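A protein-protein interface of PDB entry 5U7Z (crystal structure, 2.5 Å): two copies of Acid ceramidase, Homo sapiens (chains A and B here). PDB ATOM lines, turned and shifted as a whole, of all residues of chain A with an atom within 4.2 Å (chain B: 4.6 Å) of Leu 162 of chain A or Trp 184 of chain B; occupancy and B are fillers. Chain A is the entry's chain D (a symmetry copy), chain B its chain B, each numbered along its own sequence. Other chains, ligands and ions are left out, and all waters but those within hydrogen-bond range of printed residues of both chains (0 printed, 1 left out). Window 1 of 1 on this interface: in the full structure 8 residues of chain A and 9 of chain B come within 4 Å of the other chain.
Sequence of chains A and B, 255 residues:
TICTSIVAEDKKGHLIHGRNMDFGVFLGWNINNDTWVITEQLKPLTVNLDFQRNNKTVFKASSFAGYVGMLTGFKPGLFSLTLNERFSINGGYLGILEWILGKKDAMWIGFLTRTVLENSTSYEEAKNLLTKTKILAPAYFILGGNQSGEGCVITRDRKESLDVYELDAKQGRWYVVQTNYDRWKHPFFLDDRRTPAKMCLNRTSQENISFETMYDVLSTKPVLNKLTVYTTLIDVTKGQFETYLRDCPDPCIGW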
ATOM      1  N   ARG A  86     -43.199 -23.177  14.179  1.00  0.00           N
ATOM      2  CA  ARG A  86     -42.430 -22.007  13.780  1.00  0.00           C
ATOM      3  C   ARG A  86     -42.686 -21.744  12.305  1.00  0.00           C
ATOM      4  O   ARG A  86     -42.607 -22.664  11.484  1.00  0.00           O
ATOM      5  CB  ARG A  86     -40.933 -22.203  14.035  1.00  0.00           C
ATOM      6  CG  ARG A  86     -40.108 -20.941  13.827  1.00  0.00           C
ATOM      7  CD  ARG A  86     -38.675 -21.125  14.300  1.00  0.00           C
ATOM      8  NE  ARG A  86     -37.854 -19.949  14.021  1.00  0.00           N
ATOM      9  CZ  ARG A  86     -37.097 -19.789  12.938  1.00  0.00           C
ATOM     10  NH1 ARG A  86     -37.037 -20.733  12.009  1.00  0.00           N
ATOM     11  NH2 ARG A  86     -36.391 -18.677  12.788  1.00  0.00           N
ATOM     12  N   THR A 155     -34.808 -22.784  19.134  1.00  0.00           N
ATOM     13  CA  THR A 155     -35.365 -22.230  17.907  1.00  0.00           C
ATOM     14  C   THR A 155     -34.589 -22.795  16.725  1.00  0.00           C
ATOM     15  O   THR A 155     -33.387 -22.546  16.592  1.00  0.00           O
ATOM     16  CB  THR A 155     -35.292 -20.706  17.925  1.00  0.00           C
ATOM     17  OG1 THR A 155     -36.044 -20.198  19.035  1.00  0.00           O
ATOM     18  CG2 THR A 155     -35.837 -20.119  16.620  1.00  0.00           C
ATOM     19  N   ASP A 157     -33.889 -23.758  12.589  1.00  0.00           N
ATOM     20  CA  ASP A 157     -34.037 -23.677  11.148  1.00  0.00           C
ATOM     21  C   ASP A 157     -33.905 -25.094  10.600  1.00  0.00           C
ATOM     22  O   ASP A 157     -33.553 -26.031  11.322  1.00  0.00           O
ATOM     23  CB  ASP A 157     -32.972 -22.751  10.546  1.00  0.00           C
ATOM     24  CG  ASP A 157     -33.559 -21.693   9.631  1.00  0.00           C
ATOM     25  OD1 ASP A 157     -34.651 -21.918   9.068  1.00  0.00           O
ATOM     26  OD2 ASP A 157     -32.917 -20.632   9.471  1.00  0.00           O
ATOM     27  N   LYS A 159     -31.705 -26.481   8.828  1.00  0.00           N
ATOM     28  CA  LYS A 159     -30.361 -27.044   8.922  1.00  0.00           C
ATOM     29  C   LYS A 159     -29.491 -26.348   9.966  1.00  0.00           C
ATOM     30  O   LYS A 159     -28.268 -26.520   9.949  1.00  0.00           O
ATOM     31  CB  LYS A 159     -29.671 -27.000   7.556  1.00  0.00           C
ATOM     32  CG  LYS A 159     -30.362 -27.842   6.495  1.00  0.00           C
ATOM     33  CD  LYS A 159     -29.701 -27.711   5.130  1.00  0.00           C
ATOM     34  CE  LYS A 159     -30.557 -28.351   4.041  1.00  0.00           C
ATOM     35  NZ  LYS A 159     -29.848 -28.466   2.730  1.00  0.00           N
ATOM     36  N   GLU A 160     -30.078 -25.569  10.876  1.00  0.00           N
ATOM     37  CA  GLU A 160     -29.277 -24.827  11.842  1.00  0.00           C
ATOM     38  C   GLU A 160     -30.078 -24.567  13.107  1.00  0.00           C
ATOM     39  O   GLU A 160     -31.311 -24.493  13.081  1.00  0.00           O
ATOM     40  CB  GLU A 160     -28.795 -23.495  11.254  1.00  0.00           C
ATOM     41  CG  GLU A 160     -27.786 -22.744  12.116  1.00  0.00           C
ATOM     42  CD  GLU A 160     -26.457 -23.465  12.218  1.00  0.00           C
ATOM     43  OE1 GLU A 160     -26.191 -24.350  11.377  1.00  0.00           O
ATOM     44  OE2 GLU A 160     -25.677 -23.141  13.137  1.00  0.00           O
ATOM     45  N   SER A 161     -29.358 -24.410  14.215  1.00  0.00           N
ATOM     46  CA  SER A 161     -29.943 -24.015  15.491  1.00  0.00           C
ATOM     47  C   SER A 161     -29.636 -22.537  15.705  1.00  0.00           C
ATOM     48  O   SER A 161     -28.493 -22.168  15.993  1.00  0.00           O
ATOM     49  CB  SER A 161     -29.392 -24.865  16.633  1.00  0.00           C
ATOM     50  OG  SER A 161     -30.028 -24.538  17.856  1.00  0.00           O
ATOM     51  N   LEU A 162     -30.662 -21.694  15.560  1.00  0.00           N
ATOM     52  CA  LEU A 162     -30.465 -20.251  15.623  1.00  0.00           C
ATOM     53  C   LEU A 162     -30.247 -19.770  17.051  1.00  0.00           C
ATOM     54  O   LEU A 162     -29.569 -18.757  17.265  1.00  0.00           O
ATOM     55  CB  LEU A 162     -31.668 -19.537  15.007  1.00  0.00           C
ATOM     56  CG  LEU A 162     -32.036 -19.997  13.596  1.00  0.00           C
ATOM     57  CD1 LEU A 162     -33.316 -19.331  13.135  1.00  0.00           C
ATOM     58  CD2 LEU A 162     -30.902 -19.713  12.620  1.00  0.00           C
ATOM     59  N   ASP A 163     -30.810 -20.469  18.030  1.00  0.00           N
ATOM     60  CA  ASP A 163     -30.704 -20.045  19.418  1.00  0.00           C
ATOM     61  C   ASP A 163     -31.104 -21.200  20.321  1.00  0.00           C
ATOM     62  O   ASP A 163     -32.020 -21.961  19.997  1.00  0.00           O
ATOM     63  CB  ASP A 163     -31.593 -18.824  19.686  1.00  0.00           C
ATOM     64  CG  ASP A 163     -31.549 -18.377  21.131  1.00  0.00           C
ATOM     65  OD1 ASP A 163     -30.436 -18.226  21.679  1.00  0.00           O
ATOM     66  OD2 ASP A 163     -32.632 -18.180  21.719  1.00  0.00           O
ATOM     67  N   THR B 155     -22.933 -14.420  12.396  1.00  0.00           N
ATOM     68  CA  THR B 155     -24.146 -14.113  11.650  1.00  0.00           C
ATOM     69  C   THR B 155     -25.126 -13.431  12.597  1.00  0.00           C
ATOM     70  O   THR B 155     -25.566 -14.036  13.580  1.00  0.00           O
ATOM     71  CB  THR B 155     -24.756 -15.383  11.061  1.00  0.00           C
ATOM     72  OG1 THR B 155     -23.810 -16.007  10.184  1.00  0.00           O
ATOM     73  CG2 THR B 155     -26.025 -15.058  10.282  1.00  0.00           C
ATOM     74  N   SER B 161     -27.774 -13.073  17.887  1.00  0.00           N
ATOM     75  CA  SER B 161     -26.672 -13.710  17.173  1.00  0.00           C
ATOM     76  C   SER B 161     -27.123 -15.107  16.760  1.00  0.00           C
ATOM     77  O   SER B 161     -27.254 -15.998  17.604  1.00  0.00           O
ATOM     78  CB  SER B 161     -25.421 -13.771  18.045  1.00  0.00           C
ATOM     79  OG  SER B 161     -24.328 -14.312  17.324  1.00  0.00           O
ATOM     80  N   LEU B 162     -27.366 -15.296  15.460  1.00  0.00           N
ATOM     81  CA  LEU B 162     -27.912 -16.561  14.982  1.00  0.00           C
ATOM     82  C   LEU B 162     -26.869 -17.670  14.972  1.00  0.00           C
ATOM     83  O   LEU B 162     -27.220 -18.846  15.127  1.00  0.00           O
ATOM     84  CB  LEU B 162     -28.493 -16.387  13.579  1.00  0.00           C
ATOM     85  CG  LEU B 162     -29.515 -15.267  13.396  1.00  0.00           C
ATOM     86  CD1 LEU B 162     -29.890 -15.146  11.933  1.00  0.00           C
ATOM     87  CD2 LEU B 162     -30.750 -15.506  14.245  1.00  0.00           C
ATOM     88  N   ASP B 163     -25.596 -17.331  14.782  1.00  0.00           N
ATOM     89  CA  ASP B 163     -24.558 -18.348  14.695  1.00  0.00           C
ATOM     90  C   ASP B 163     -23.194 -17.693  14.838  1.00  0.00           C
ATOM     91  O   ASP B 163     -22.981 -16.584  14.341  1.00  0.00           O
ATOM     92  CB  ASP B 163     -24.645 -19.103  13.362  1.00  0.00           C
ATOM     93  CG  ASP B 163     -23.552 -20.138  13.208  1.00  0.00           C
ATOM     94  OD1 ASP B 163     -23.349 -20.939  14.144  1.00  0.00           O
ATOM     95  OD2 ASP B 163     -22.892 -20.149  12.149  1.00  0.00           O
ATOM     96  N   ASP B 182     -26.332 -16.922   4.311  1.00  0.00           N
ATOM     97  CA  ASP B 182     -26.129 -17.700   5.526  1.00  0.00           C
ATOM     98  C   ASP B 182     -25.531 -19.065   5.201  1.00  0.00           C
ATOM     99  O   ASP B 182     -25.944 -19.736   4.251  1.00  0.00           O
ATOM    100  CB  ASP B 182     -27.453 -17.855   6.272  1.00  0.00           C
ATOM    101  CG  ASP B 182     -27.972 -16.536   6.811  1.00  0.00           C
ATOM    102  OD1 ASP B 182     -27.156 -15.609   7.005  1.00  0.00           O
ATOM    103  OD2 ASP B 182     -29.194 -16.422   7.037  1.00  0.00           O
ATOM    104  N   ARG B 183     -24.560 -19.479   6.019  1.00  0.00           N
ATOM    105  CA  ARG B 183     -23.762 -20.662   5.707  1.00  0.00           C
ATOM    106  C   ARG B 183     -24.627 -21.904   5.526  1.00  0.00           C
ATOM    107  O   ARG B 183     -24.371 -22.723   4.636  1.00  0.00           O
ATOM    108  CB  ARG B 183     -22.738 -20.896   6.818  1.00  0.00           C
ATOM    109  CG  ARG B 183     -21.776 -22.049   6.544  1.00  0.00           C
ATOM    110  CD  ARG B 183     -20.913 -22.407   7.756  1.00  0.00           C
ATOM    111  NE  ARG B 183     -21.480 -21.942   9.022  1.00  0.00           N
ATOM    112  CZ  ARG B 183     -22.266 -22.667   9.813  1.00  0.00           C
ATOM    113  NH1 ARG B 183     -22.600 -23.911   9.488  1.00  0.00           N
ATOM    114  NH2 ARG B 183     -22.724 -22.146  10.943  1.00  0.00           N
ATOM    115  N   TRP B 184     -25.645 -22.069   6.367  1.00  0.00           N
ATOM    116  CA  TRP B 184     -26.482 -23.261   6.344  1.00  0.00           C
ATOM    117  C   TRP B 184     -27.569 -23.212   5.278  1.00  0.00           C
ATOM    118  O   TRP B 184     -28.376 -24.145   5.203  1.00  0.00           O
ATOM    119  CB  TRP B 184     -27.127 -23.478   7.716  1.00  0.00           C
ATOM    120  CG  TRP B 184     -27.969 -22.326   8.167  1.00  0.00           C
ATOM    121  CD1 TRP B 184     -29.317 -22.192   8.022  1.00  0.00           C
ATOM    122  CD2 TRP B 184     -27.518 -21.147   8.846  1.00  0.00           C
ATOM    123  NE1 TRP B 184     -29.734 -21.000   8.563  1.00  0.00           N
ATOM    124  CE2 TRP B 184     -28.649 -20.340   9.075  1.00  0.00           C
ATOM    125  CE3 TRP B 184     -26.266 -20.695   9.279  1.00  0.00           C
ATOM    126  CZ2 TRP B 184     -28.567 -19.108   9.716  1.00  0.00           C
ATOM    127  CZ3 TRP B 184     -26.188 -19.472   9.914  1.00  0.00           C
ATOM    128  CH2 TRP B 184     -27.330 -18.693  10.129  1.00  0.00           C
ATOM    129  N   LYS B 185     -27.621 -22.161   4.462  1.00  0.00           N
ATOM    130  CA  LYS B 185     -28.635 -22.011   3.434  1.00  0.00           C
ATOM    131  C   LYS B 185     -27.992 -22.144   2.049  1.00  0.00           C
ATOM    132  O   LYS B 185     -26.970 -22.838   1.905  1.00  0.00           O
ATOM    133  CB  LYS B 185     -29.366 -20.690   3.649  1.00  0.00           C
ATOM    134  CG  LYS B 185     -29.933 -20.538   5.043  1.00  0.00           C
ATOM    135  CD  LYS B 185     -31.186 -19.693   5.021  1.00  0.00           C
ATOM    136  CE  LYS B 185     -31.931 -19.797   6.333  1.00  0.00           C
ATOM    137  NZ  LYS B 185     -33.106 -18.892   6.374  1.00  0.00           N
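Hydrophobic or aromatic side chains of chain B within 4 Å of the printed part of chain A: Trp 184. Printed residues of chain A that touch a printed residue of chain B: Asp 157, Lys 159, Glu 160, Ser 161 and Leu 162. Among the printed residues, 10 pairs touch across the chains.
Printed residues of chain B within 4 Å of Ser 161 of chain A: Leu 162. Printed residues of chain A within 4 Å of Lys 185 of chain B: Asp 157. The nearest printed residue of chain B that does not touch Leu 162 of chain A is Asp 163 of chain B (4.9 Å). The nearest printed residue of chain A that does not touch Trp 184 of chain B is Ser 161 of chain A (6.5 Å).
Ser 161 of chain A touches Leu 162 of chain B, and with the chains exchanged Leu 162 of chain A touches Ser 161 of chain B. Leu 162 of chain A touches its own counterpart, Leu 162 of chain B. 4 positions are printed for both chains. Of the 10 pairs that touch across the chains among the printed residues, 3 have their exchanged pair printed and touching as well.
O of Thr 155 of chain B sits at hydrogen-bond distance from N of Leu 162 of chain B (2.9 Å). The backbone carbonyl oxygen (O) of Asp 163 of chain B sits at hydrogen-bond distance from the backbone NH (N) of Thr 155 of chain B (2.9 Å). The side-chain carboxylate (OD1) of Asp 163 of chain B is in salt-bridge range of the guanidinium group (NH2) of Arg 183 of chain B. The guanidinium group (NH1) of Arg 86 of chain A lies within salt-bridge range of the side-chain carboxylate (OD1) of Asp 157 of chain A, at 3.97 Å. O of Thr 155 of chain A lies within hydrogen-bond range of N of Leu 162 of chain A.
Among the printed residues, merely in contact across the chains: Lys 159 of chain A with Trp 184 of chain B, Glu 160 of chain A with Trp 184 of chain B, Ser 161 of chain A with Leu 162 of chain B, Leu 162 of chain A with Ser 161 of chain B and Leu 162 of chain A with Trp 184 of chain B.
The guanidinium group of Arg 183 of chain B lies within salt-bridge range of the side-chain carboxylate of Glu 160 of chain A, 3.8 Å away. The side-chain carboxylate (OD2) of Asp 157 of chain A lies within hydrogen-bond range of the indole nitrogen (NE1) of Trp 184 of chain B (3.3 Å). The side-chain amino group of Lys 185 of chain B lies within salt-bridge range of the side-chain carboxylate of Asp 157 of chain A. OE2 of Glu 160 of chain A sits close to OD1 of Asp 163 of chain B (3.4 Å). The backbone carbonyl oxygen (O) of Leu 162 of chain A lies close to the backbone carbonyl oxygen (O) of Leu 162 of chain B (3.2 Å).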
